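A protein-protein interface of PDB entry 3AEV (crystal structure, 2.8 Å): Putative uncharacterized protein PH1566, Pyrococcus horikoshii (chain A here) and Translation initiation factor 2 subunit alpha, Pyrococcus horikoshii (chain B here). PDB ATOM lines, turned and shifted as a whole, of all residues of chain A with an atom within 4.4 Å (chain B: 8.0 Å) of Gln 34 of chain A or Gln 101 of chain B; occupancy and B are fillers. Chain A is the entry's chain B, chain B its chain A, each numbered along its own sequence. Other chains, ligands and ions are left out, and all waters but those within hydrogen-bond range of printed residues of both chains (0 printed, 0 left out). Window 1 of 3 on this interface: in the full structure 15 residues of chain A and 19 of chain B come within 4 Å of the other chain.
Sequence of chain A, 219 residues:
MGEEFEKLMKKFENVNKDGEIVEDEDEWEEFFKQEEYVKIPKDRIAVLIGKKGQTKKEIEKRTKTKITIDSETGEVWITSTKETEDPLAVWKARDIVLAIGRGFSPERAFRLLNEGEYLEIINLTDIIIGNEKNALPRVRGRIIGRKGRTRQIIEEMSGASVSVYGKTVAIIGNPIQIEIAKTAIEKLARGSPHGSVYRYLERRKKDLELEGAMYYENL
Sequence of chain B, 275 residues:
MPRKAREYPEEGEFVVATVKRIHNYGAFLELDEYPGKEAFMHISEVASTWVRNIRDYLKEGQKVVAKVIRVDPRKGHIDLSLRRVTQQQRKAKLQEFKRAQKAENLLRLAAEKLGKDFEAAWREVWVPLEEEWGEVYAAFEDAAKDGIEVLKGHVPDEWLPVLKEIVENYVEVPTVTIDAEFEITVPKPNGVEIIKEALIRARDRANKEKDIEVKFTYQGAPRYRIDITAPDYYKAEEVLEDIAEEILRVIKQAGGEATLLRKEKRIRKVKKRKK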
ATOM      1  N   PHE A  31     -22.513  -8.517  11.167  1.00  0.00           N
ATOM      2  CA  PHE A  31     -21.788  -9.245  12.211  1.00  0.00           C
ATOM      3  C   PHE A  31     -21.856 -10.767  12.074  1.00  0.00           C
ATOM      4  O   PHE A  31     -21.048 -11.485  12.664  1.00  0.00           O
ATOM      5  CB  PHE A  31     -22.286  -8.852  13.608  1.00  0.00           C
ATOM      6  CG  PHE A  31     -21.937  -7.460  14.014  1.00  0.00           C
ATOM      7  CD1 PHE A  31     -20.866  -7.221  14.854  1.00  0.00           C
ATOM      8  CD2 PHE A  31     -22.693  -6.381  13.576  1.00  0.00           C
ATOM      9  CE1 PHE A  31     -20.538  -5.943  15.246  1.00  0.00           C
ATOM     10  CE2 PHE A  31     -22.373  -5.089  13.963  1.00  0.00           C
ATOM     11  CZ  PHE A  31     -21.294  -4.869  14.806  1.00  0.00           C
ATOM     12  N   PHE A  32     -22.817 -11.282  11.317  1.00  0.00           N
ATOM     13  CA  PHE A  32     -22.983 -12.730  11.307  1.00  0.00           C
ATOM     14  C   PHE A  32     -23.040 -13.462   9.963  1.00  0.00           C
ATOM     15  O   PHE A  32     -22.608 -14.612   9.869  1.00  0.00           O
ATOM     16  CB  PHE A  32     -24.165 -13.121  12.183  1.00  0.00           C
ATOM     17  CG  PHE A  32     -24.054 -12.648  13.611  1.00  0.00           C
ATOM     18  CD1 PHE A  32     -24.883 -11.625  14.079  1.00  0.00           C
ATOM     19  CD2 PHE A  32     -23.143 -13.246  14.491  1.00  0.00           C
ATOM     20  CE1 PHE A  32     -24.813 -11.205  15.387  1.00  0.00           C
ATOM     21  CE2 PHE A  32     -23.053 -12.831  15.818  1.00  0.00           C
ATOM     22  CZ  PHE A  32     -23.892 -11.809  16.267  1.00  0.00           C
ATOM     23  N   LYS A  33     -23.569 -12.810   8.941  1.00  0.00           N
ATOM     24  CA  LYS A  33     -23.692 -13.395   7.604  1.00  0.00           C
ATOM     25  C   LYS A  33     -22.385 -14.073   7.133  1.00  0.00           C
ATOM     26  O   LYS A  33     -21.310 -13.446   7.110  1.00  0.00           O
ATOM     27  CB  LYS A  33     -24.157 -12.324   6.588  1.00  0.00           C
ATOM     28  CG  LYS A  33     -24.540 -12.891   5.226  1.00  0.00           C
ATOM     29  CD  LYS A  33     -25.321 -11.914   4.360  1.00  0.00           C
ATOM     30  CE  LYS A  33     -24.387 -11.125   3.455  1.00  0.00           C
ATOM     31  NZ  LYS A  33     -25.112 -10.161   2.571  1.00  0.00           N
ATOM     32  N   GLN A  34     -22.469 -15.351   6.785  1.00  0.00           N
ATOM     33  CA  GLN A  34     -21.342 -15.979   6.091  1.00  0.00           C
ATOM     34  C   GLN A  34     -21.661 -16.012   4.598  1.00  0.00           C
ATOM     35  O   GLN A  34     -22.787 -16.313   4.218  1.00  0.00           O
ATOM     36  CB  GLN A  34     -21.012 -17.382   6.641  1.00  0.00           C
ATOM     37  CG  GLN A  34     -20.596 -17.443   8.136  1.00  0.00           C
ATOM     38  CD  GLN A  34     -19.286 -16.662   8.507  1.00  0.00           C
ATOM     39  OE1 GLN A  34     -19.042 -16.359   9.692  1.00  0.00           O
ATOM     40  NE2 GLN A  34     -18.450 -16.358   7.499  1.00  0.00           N
ATOM     41  N   GLU A  35     -20.690 -15.663   3.761  1.00  0.00           N
ATOM     42  CA  GLU A  35     -20.912 -15.671   2.329  1.00  0.00           C
ATOM     43  C   GLU A  35     -19.757 -16.291   1.587  1.00  0.00           C
ATOM     44  O   GLU A  35     -18.600 -16.059   1.904  1.00  0.00           O
ATOM     45  CB  GLU A  35     -21.246 -14.275   1.772  1.00  0.00           C
ATOM     46  CG  GLU A  35     -20.223 -13.180   2.029  1.00  0.00           C
ATOM     47  CD  GLU A  35     -20.842 -11.757   2.031  1.00  0.00           C
ATOM     48  OE1 GLU A  35     -20.943 -11.119   3.128  1.00  0.00           O
ATOM     49  OE2 GLU A  35     -21.226 -11.280   0.932  1.00  0.00           O
ATOM     50  N   ILE A  78     -23.502 -17.744  -2.303  1.00  0.00           N
ATOM     51  CA  ILE A  78     -24.190 -18.516  -1.295  1.00  0.00           C
ATOM     52  C   ILE A  78     -24.056 -17.799   0.041  1.00  0.00           C
ATOM     53  O   ILE A  78     -22.938 -17.518   0.481  1.00  0.00           O
ATOM     54  CB  ILE A  78     -23.542 -19.920  -1.139  1.00  0.00           C
ATOM     55  CG1 ILE A  78     -23.471 -20.675  -2.464  1.00  0.00           C
ATOM     56  CG2 ILE A  78     -24.301 -20.771  -0.131  1.00  0.00           C
ATOM     57  CD1 ILE A  78     -22.178 -20.479  -3.175  1.00  0.00           C
ATOM     58  N   THR A  79     -25.167 -17.497   0.702  1.00  0.00           N
ATOM     59  CA  THR A  79     -25.073 -16.866   2.020  1.00  0.00           C
ATOM     60  C   THR A  79     -25.941 -17.545   3.077  1.00  0.00           C
ATOM     61  O   THR A  79     -26.896 -18.228   2.753  1.00  0.00           O
ATOM     62  CB  THR A  79     -25.404 -15.360   1.971  1.00  0.00           C
ATOM     63  OG1 THR A  79     -26.822 -15.173   2.028  1.00  0.00           O
ATOM     64  CG2 THR A  79     -24.825 -14.689   0.712  1.00  0.00           C
ATOM     65  N   SER A  80     -25.595 -17.362   4.344  1.00  0.00           N
ATOM     66  CA  SER A  80     -26.447 -17.816   5.428  1.00  0.00           C
ATOM     67  C   SER A  80     -27.704 -16.961   5.464  1.00  0.00           C
ATOM     68  O   SER A  80     -27.799 -15.971   4.723  1.00  0.00           O
ATOM     69  CB  SER A  80     -25.713 -17.750   6.777  1.00  0.00           C
ATOM     70  OG  SER A  80     -24.956 -16.551   6.954  1.00  0.00           O
ATOM     71  N   VAL A  90     -23.297 -23.217   4.823  1.00  0.00           N
ATOM     72  CA  VAL A  90     -22.914 -22.408   3.678  1.00  0.00           C
ATOM     73  C   VAL A  90     -21.907 -23.185   2.858  1.00  0.00           C
ATOM     74  O   VAL A  90     -22.016 -23.257   1.644  1.00  0.00           O
ATOM     75  CB  VAL A  90     -22.355 -21.042   4.098  1.00  0.00           C
ATOM     76  CG1 VAL A  90     -21.707 -20.329   2.931  1.00  0.00           C
ATOM     77  CG2 VAL A  90     -23.464 -20.187   4.681  1.00  0.00           C
ATOM     78  N   TRP A  91     -20.953 -23.806   3.536  1.00  0.00           N
ATOM     79  CA  TRP A  91     -19.923 -24.576   2.870  1.00  0.00           C
ATOM     80  C   TRP A  91     -20.454 -25.829   2.163  1.00  0.00           C
ATOM     81  O   TRP A  91     -20.062 -26.125   1.030  1.00  0.00           O
ATOM     82  CB  TRP A  91     -18.795 -24.865   3.848  1.00  0.00           C
ATOM     83  CG  TRP A  91     -18.181 -23.566   4.256  1.00  0.00           C
ATOM     84  CD1 TRP A  91     -17.128 -22.948   3.660  1.00  0.00           C
ATOM     85  CD2 TRP A  91     -18.644 -22.674   5.293  1.00  0.00           C
ATOM     86  NE1 TRP A  91     -16.898 -21.739   4.262  1.00  0.00           N
ATOM     87  CE2 TRP A  91     -17.805 -21.545   5.269  1.00  0.00           C
ATOM     88  CE3 TRP A  91     -19.698 -22.720   6.231  1.00  0.00           C
ATOM     89  CZ2 TRP A  91     -17.964 -20.459   6.154  1.00  0.00           C
ATOM     90  CZ3 TRP A  91     -19.852 -21.634   7.124  1.00  0.00           C
ATOM     91  CH2 TRP A  91     -18.975 -20.523   7.075  1.00  0.00           C
ATOM     92  N   VAL B  16     -16.048  -6.269  19.798  1.00  0.00           N
ATOM     93  CA  VAL B  16     -17.458  -6.211  19.454  1.00  0.00           C
ATOM     94  C   VAL B  16     -18.182  -6.046  20.785  1.00  0.00           C
ATOM     95  O   VAL B  16     -17.880  -6.722  21.745  1.00  0.00           O
ATOM     96  CB  VAL B  16     -17.900  -7.515  18.702  1.00  0.00           C
ATOM     97  CG1 VAL B  16     -19.428  -7.596  18.487  1.00  0.00           C
ATOM     98  CG2 VAL B  16     -17.183  -7.627  17.371  1.00  0.00           C
ATOM     99  N   LEU B  94     -14.378  -6.807  11.791  1.00  0.00           N
ATOM    100  CA  LEU B  94     -15.574  -7.504  11.483  1.00  0.00           C
ATOM    101  C   LEU B  94     -15.199  -8.765  10.711  1.00  0.00           C
ATOM    102  O   LEU B  94     -15.799  -9.831  10.920  1.00  0.00           O
ATOM    103  CB  LEU B  94     -16.419  -6.573  10.645  1.00  0.00           C
ATOM    104  CG  LEU B  94     -17.827  -6.265  11.103  1.00  0.00           C
ATOM    105  CD1 LEU B  94     -18.009  -6.302  12.631  1.00  0.00           C
ATOM    106  CD2 LEU B  94     -18.172  -4.919  10.505  1.00  0.00           C
ATOM    107  N   GLN B  95     -14.202  -8.660   9.830  1.00  0.00           N
ATOM    108  CA  GLN B  95     -13.664  -9.841   9.175  1.00  0.00           C
ATOM    109  C   GLN B  95     -13.110 -10.798  10.224  1.00  0.00           C
ATOM    110  O   GLN B  95     -13.419 -12.005  10.216  1.00  0.00           O
ATOM    111  CB  GLN B  95     -12.594  -9.468   8.183  1.00  0.00           C
ATOM    112  CG  GLN B  95     -13.140  -9.172   6.838  1.00  0.00           C
ATOM    113  CD  GLN B  95     -12.116  -8.488   5.957  1.00  0.00           C
ATOM    114  OE1 GLN B  95     -11.920  -7.278   6.049  1.00  0.00           O
ATOM    115  NE2 GLN B  95     -11.461  -9.255   5.095  1.00  0.00           N
ATOM    116  N   GLU B  96     -12.328 -10.254  11.154  1.00  0.00           N
ATOM    117  CA  GLU B  96     -11.687 -11.075  12.166  1.00  0.00           C
ATOM    118  C   GLU B  96     -12.747 -11.758  13.037  1.00  0.00           C
ATOM    119  O   GLU B  96     -12.596 -12.914  13.359  1.00  0.00           O
ATOM    120  CB  GLU B  96     -10.640 -10.254  12.934  1.00  0.00           C
ATOM    121  CG  GLU B  96     -10.123 -10.821  14.253  1.00  0.00           C
ATOM    122  CD  GLU B  96      -9.445  -9.729  15.168  1.00  0.00           C
ATOM    123  OE1 GLU B  96      -8.559  -8.964  14.675  1.00  0.00           O
ATOM    124  OE2 GLU B  96      -9.808  -9.614  16.378  1.00  0.00           O
ATOM    125  N   PHE B  97     -13.853 -11.087  13.334  1.00  0.00           N
ATOM    126  CA  PHE B  97     -14.914 -11.636  14.183  1.00  0.00           C
ATOM    127  C   PHE B  97     -15.574 -12.757  13.428  1.00  0.00           C
ATOM    128  O   PHE B  97     -15.829 -13.801  14.009  1.00  0.00           O
ATOM    129  CB  PHE B  97     -15.914 -10.525  14.523  1.00  0.00           C
ATOM    130  CG  PHE B  97     -17.078 -10.917  15.430  1.00  0.00           C
ATOM    131  CD1 PHE B  97     -18.383 -10.849  14.965  1.00  0.00           C
ATOM    132  CD2 PHE B  97     -16.896 -11.197  16.770  1.00  0.00           C
ATOM    133  CE1 PHE B  97     -19.471 -11.130  15.817  1.00  0.00           C
ATOM    134  CE2 PHE B  97     -17.982 -11.481  17.617  1.00  0.00           C
ATOM    135  CZ  PHE B  97     -19.260 -11.455  17.138  1.00  0.00           C
ATOM    136  N   LYS B  98     -15.828 -12.576  12.132  1.00  0.00           N
ATOM    137  CA  LYS B  98     -16.478 -13.635  11.333  1.00  0.00           C
ATOM    138  C   LYS B  98     -15.613 -14.895  11.161  1.00  0.00           C
ATOM    139  O   LYS B  98     -16.133 -16.015  11.013  1.00  0.00           O
ATOM    140  CB  LYS B  98     -16.901 -13.100   9.968  1.00  0.00           C
ATOM    141  CG  LYS B  98     -17.976 -12.004  10.039  1.00  0.00           C
ATOM    142  CD  LYS B  98     -18.795 -11.880   8.773  1.00  0.00           C
ATOM    143  CE  LYS B  98     -20.012 -11.013   9.049  1.00  0.00           C
ATOM    144  NZ  LYS B  98     -20.732 -10.589   7.803  1.00  0.00           N
ATOM    145  N   ARG B  99     -14.293 -14.706  11.185  1.00  0.00           N
ATOM    146  CA  ARG B  99     -13.380 -15.815  11.081  1.00  0.00           C
ATOM    147  C   ARG B  99     -13.321 -16.539  12.419  1.00  0.00           C
ATOM    148  O   ARG B  99     -13.138 -17.766  12.460  1.00  0.00           O
ATOM    149  CB  ARG B  99     -11.996 -15.358  10.632  1.00  0.00           C
ATOM    150  CG  ARG B  99     -11.854 -14.994   9.142  1.00  0.00           C
ATOM    151  CD  ARG B  99     -10.734 -13.948   8.899  1.00  0.00           C
ATOM    152  NE  ARG B  99      -9.413 -14.269   9.475  1.00  0.00           N
ATOM    153  CZ  ARG B  99      -8.438 -14.939   8.842  1.00  0.00           C
ATOM    154  NH1 ARG B  99      -8.617 -15.391   7.612  1.00  0.00           N
ATOM    155  NH2 ARG B  99      -7.270 -15.180   9.438  1.00  0.00           N
ATOM    156  N   ALA B 100     -13.487 -15.806  13.521  1.00  0.00           N
ATOM    157  CA  ALA B 100     -13.527 -16.480  14.820  1.00  0.00           C
ATOM    158  C   ALA B 100     -14.797 -17.330  14.976  1.00  0.00           C
ATOM    159  O   ALA B 100     -14.754 -18.354  15.649  1.00  0.00           O
ATOM    160  CB  ALA B 100     -13.372 -15.511  15.955  1.00  0.00           C
ATOM    161  N   GLN B 101     -15.915 -16.928  14.359  1.00  0.00           N
ATOM    162  CA  GLN B 101     -17.114 -17.785  14.339  1.00  0.00           C
ATOM    163  C   GLN B 101     -16.868 -19.066  13.523  1.00  0.00           C
ATOM    164  O   GLN B 101     -17.366 -20.115  13.885  1.00  0.00           O
ATOM    165  CB  GLN B 101     -18.373 -17.072  13.823  1.00  0.00           C
ATOM    166  CG  GLN B 101     -18.962 -15.940  14.716  1.00  0.00           C
ATOM    167  CD  GLN B 101     -19.910 -14.952  13.917  1.00  0.00           C
ATOM    168  OE1 GLN B 101     -19.805 -13.722  14.047  1.00  0.00           O
ATOM    169  NE2 GLN B 101     -20.821 -15.518  13.078  1.00  0.00           N
ATOM    170  N   LYS B 102     -16.103 -18.978  12.433  1.00  0.00           N
ATOM    171  CA  LYS B 102     -15.777 -20.165  11.648  1.00  0.00           C
ATOM    172  C   LYS B 102     -14.878 -21.089  12.460  1.00  0.00           C
ATOM    173  O   LYS B 102     -15.096 -22.307  12.550  1.00  0.00           O
ATOM    174  CB  LYS B 102     -15.059 -19.788  10.362  1.00  0.00           C
ATOM    175  CG  LYS B 102     -15.975 -19.647   9.160  1.00  0.00           C
ATOM    176  CD  LYS B 102     -15.205 -19.674   7.802  1.00  0.00           C
ATOM    177  CE  LYS B 102     -14.953 -18.260   7.205  1.00  0.00           C
ATOM    178  NZ  LYS B 102     -14.884 -18.300   5.707  1.00  0.00           N
ATOM    179  N   ALA B 103     -13.851 -20.519  13.065  1.00  0.00           N
ATOM    180  CA  ALA B 103     -12.944 -21.373  13.733  1.00  0.00           C
ATOM    181  C   ALA B 103     -13.717 -22.100  14.810  1.00  0.00           C
ATOM    182  O   ALA B 103     -13.579 -23.309  14.951  1.00  0.00           O
ATOM    183  CB  ALA B 103     -11.793 -20.616  14.279  1.00  0.00           C
ATOM    184  N   GLU B 104     -14.567 -21.388  15.531  1.00  0.00           N
ATOM    185  CA  GLU B 104     -15.307 -22.014  16.623  1.00  0.00           C
ATOM    186  C   GLU B 104     -16.213 -23.151  16.152  1.00  0.00           C
ATOM    187  O   GLU B 104     -16.328 -24.188  16.812  1.00  0.00           O
ATOM    188  CB  GLU B 104     -16.117 -20.984  17.379  1.00  0.00           C
ATOM    189  CG  GLU B 104     -16.862 -21.560  18.548  1.00  0.00           C
ATOM    190  CD  GLU B 104     -17.686 -20.517  19.269  1.00  0.00           C
ATOM    191  OE1 GLU B 104     -17.080 -19.593  19.866  1.00  0.00           O
ATOM    192  OE2 GLU B 104     -18.938 -20.632  19.246  1.00  0.00           O
ATOM    193  N   ASN B 105     -16.834 -22.960  14.997  1.00  0.00           N
ATOM    194  CA  ASN B 105     -17.694 -23.975  14.420  1.00  0.00           C
ATOM    195  C   ASN B 105     -16.912 -25.173  13.943  1.00  0.00           C
ATOM    196  O   ASN B 105     -17.376 -26.329  14.069  1.00  0.00           O
ATOM    197  CB  ASN B 105     -18.514 -23.380  13.296  1.00  0.00           C
ATOM    198  CG  ASN B 105     -19.585 -22.455  13.827  1.00  0.00           C
ATOM    199  OD1 ASN B 105     -20.159 -22.695  14.906  1.00  0.00           O
ATOM    200  ND2 ASN B 105     -19.856 -21.387  13.091  1.00  0.00           N
ATOM    201  N   LEU B 106     -15.726 -24.900  13.396  1.00  0.00           N
ATOM    202  CA  LEU B 106     -14.850 -25.959  12.976  1.00  0.00           C
ATOM    203  C   LEU B 106     -14.416 -26.754  14.194  1.00  0.00           C
ATOM    204  O   LEU B 106     -14.443 -27.990  14.187  1.00  0.00           O
ATOM    205  CB  LEU B 106     -13.674 -25.370  12.258  1.00  0.00           C
ATOM    206  CG  LEU B 106     -13.723 -25.428  10.740  1.00  0.00           C
ATOM    207  CD1 LEU B 106     -15.106 -25.639  10.174  1.00  0.00           C
ATOM    208  CD2 LEU B 106     -13.045 -24.190  10.166  1.00  0.00           C
ATOM    209  N   LEU B 107     -14.083 -26.057  15.263  1.00  0.00           N
ATOM    210  CA  LEU B 107     -13.651 -26.742  16.468  1.00  0.00           C
ATOM    211  C   LEU B 107     -14.792 -27.555  17.111  1.00  0.00           C
ATOM    212  O   LEU B 107     -14.554 -28.676  17.565  1.00  0.00           O
ATOM    213  CB  LEU B 107     -13.002 -25.767  17.451  1.00  0.00           C
ATOM    214  CG  LEU B 107     -12.521 -26.357  18.768  1.00  0.00           C
ATOM    215  CD1 LEU B 107     -11.620 -27.610  18.574  1.00  0.00           C
ATOM    216  CD2 LEU B 107     -11.823 -25.305  19.584  1.00  0.00           C
ATOM    217  N   ARG B 108     -16.017 -27.018  17.120  1.00  0.00           N
ATOM    218  CA  ARG B 108     -17.173 -27.764  17.646  1.00  0.00           C
ATOM    219  C   ARG B 108     -17.419 -29.027  16.880  1.00  0.00           C
ATOM    220  O   ARG B 108     -17.820 -30.035  17.439  1.00  0.00           O
ATOM    221  CB  ARG B 108     -18.444 -26.955  17.575  1.00  0.00           C
ATOM    222  CG  ARG B 108     -18.567 -25.980  18.704  1.00  0.00           C
ATOM    223  CD  ARG B 108     -19.887 -25.273  18.661  1.00  0.00           C
ATOM    224  NE  ARG B 108     -19.814 -24.027  19.419  1.00  0.00           N
ATOM    225  CZ  ARG B 108     -19.922 -23.940  20.746  1.00  0.00           C
ATOM    226  NH1 ARG B 108     -19.848 -22.750  21.343  1.00  0.00           N
ATOM    227  NH2 ARG B 108     -20.093 -25.037  21.483  1.00  0.00           N
ATOM    228  N   TRP B 126      -8.445 -24.413  21.667  1.00  0.00           N
ATOM    229  CA  TRP B 126      -8.665 -22.986  21.407  1.00  0.00           C
ATOM    230  C   TRP B 126      -7.633 -22.137  22.124  1.00  0.00           C
ATOM    231  O   TRP B 126      -6.867 -21.411  21.505  1.00  0.00           O
ATOM    232  CB  TRP B 126     -10.094 -22.565  21.752  1.00  0.00           C
ATOM    233  CG  TRP B 126     -10.446 -21.168  21.294  1.00  0.00           C
ATOM    234  CD1 TRP B 126     -10.180 -19.985  21.961  1.00  0.00           C
ATOM    235  CD2 TRP B 126     -11.138 -20.791  20.080  1.00  0.00           C
ATOM    236  NE1 TRP B 126     -10.642 -18.916  21.230  1.00  0.00           N
ATOM    237  CE2 TRP B 126     -11.245 -19.369  20.085  1.00  0.00           C
ATOM    238  CE3 TRP B 126     -11.669 -21.514  18.986  1.00  0.00           C
ATOM    239  CZ2 TRP B 126     -11.868 -18.653  19.046  1.00  0.00           C
ATOM    240  CZ3 TRP B 126     -12.290 -20.793  17.939  1.00  0.00           C
ATOM    241  CH2 TRP B 126     -12.381 -19.373  17.990  1.00  0.00           C
ATOM    242  N   GLU B 135      -4.759 -15.566  16.456  1.00  0.00           N
ATOM    243  CA  GLU B 135      -6.090 -15.783  15.920  1.00  0.00           C
ATOM    244  C   GLU B 135      -6.157 -17.291  15.615  1.00  0.00           C
ATOM    245  O   GLU B 135      -5.327 -17.819  14.870  1.00  0.00           O
ATOM    246  CB  GLU B 135      -6.284 -14.885  14.677  1.00  0.00           C
ATOM    247  CG  GLU B 135      -7.406 -15.296  13.742  1.00  0.00           C
ATOM    248  CD  GLU B 135      -7.725 -14.278  12.581  1.00  0.00           C
ATOM    249  OE1 GLU B 135      -6.772 -13.724  11.959  1.00  0.00           O
ATOM    250  OE2 GLU B 135      -8.948 -14.087  12.264  1.00  0.00           O
ATOM    251  N   TYR B 137      -8.275 -18.915  13.752  1.00  0.00           N
ATOM    252  CA  TYR B 137      -8.403 -19.152  12.302  1.00  0.00           C
ATOM    253  C   TYR B 137      -7.034 -19.149  11.610  1.00  0.00           C
ATOM    254  O   TYR B 137      -6.822 -19.885  10.647  1.00  0.00           O
ATOM    255  CB  TYR B 137      -9.371 -18.196  11.599  1.00  0.00           C
ATOM    256  CG  TYR B 137      -9.945 -18.772  10.303  1.00  0.00           C
ATOM    257  CD1 TYR B 137     -10.955 -19.753  10.323  1.00  0.00           C
ATOM    258  CD2 TYR B 137      -9.470 -18.347   9.051  1.00  0.00           C
ATOM    259  CE1 TYR B 137     -11.478 -20.289   9.127  1.00  0.00           C
ATOM    260  CE2 TYR B 137      -9.980 -18.868   7.858  1.00  0.00           C
ATOM    261  CZ  TYR B 137     -10.981 -19.854   7.887  1.00  0.00           C
ATOM    262  OH  TYR B 137     -11.476 -20.380   6.676  1.00  0.00           O
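The backbone carbonyl oxygen (O) of Gln 101 of chain B lies within hydrogen-bond range of the side-chain amide nitrogen (ND2) of Asn 105 of chain B (2.9 Å). The side-chain hydroxyl (OG) of Ser 80 of chain A is in hydrogen-bond range of the backbone NH (N) of Gln 34 of chain A, at 2.8 Å.
Of the printed residues of chain A, Val 16 of chain B touches Phe 31. Of the printed residues of chain A, Phe 97 of chain B touches Phe 31 (3.5 Å) and Phe 32 (3.97 Å). Of the printed residues of chain A, Lys 102 of chain B touches Gln 34 (3.99 Å) and Trp 91 (3.3 Å). Ala 103 of chain B touches none of the printed residues of chain A. The nearest printed residue of chain B that does not touch Gln 34 of chain A is Arg 99 of chain B (5.2 Å). The nearest printed residue of chain B that does not touch Lys 33 of chain A is Gln 101 of chain B (5.7 Å).
O of Lys 33 of chain A is in hydrogen-bond range of NZ of Lys 98 of chain B (3.0 Å). The backbone carbonyl oxygen (O) of Lys 98 of chain B sits close to the side-chain amide oxygen (OE1) of Gln 34 of chain A (3.2 Å). OE1 of Gln 101 of chain B lies close to O of Phe 31 of chain A.
Val 16 of chain B touches Phe 31 of chain A (CG1 to CE1, 3.8 Å). Phe 31 of chain A touches Leu 94 of chain B. O of Phe 31 of chain A touches CE1 of Phe 97 of chain B (3.5 Å). C of Phe 31 of chain A touches CE of Lys 98 of chain B, at 3.6 Å. Phe 32 of chain A touches Phe 97 of chain B. Lys 98 of chain B touches Phe 32 of chain A. Gln 101 of chain B touches Phe 32 of chain A. Gln 101 of chain B touches Gln 34 of chain A. Gln 34 of chain A touches Lys 102 of chain B (NE2 to CE, 3.99 Å). Lys 102 of chain B touches Trp 91 of chain A.
Of the 19 printed residues of chain B, 6 touch a printed residue of chain A. Hydrophobic or aromatic side chains of chain B within 4 Å of the printed part of chain A: Val 16, Leu 94 and Phe 97. Among the printed residues, no Asp or Glu carboxylate lies within 4 Å of a Lys or Arg side-chain nitrogen of the other chain.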
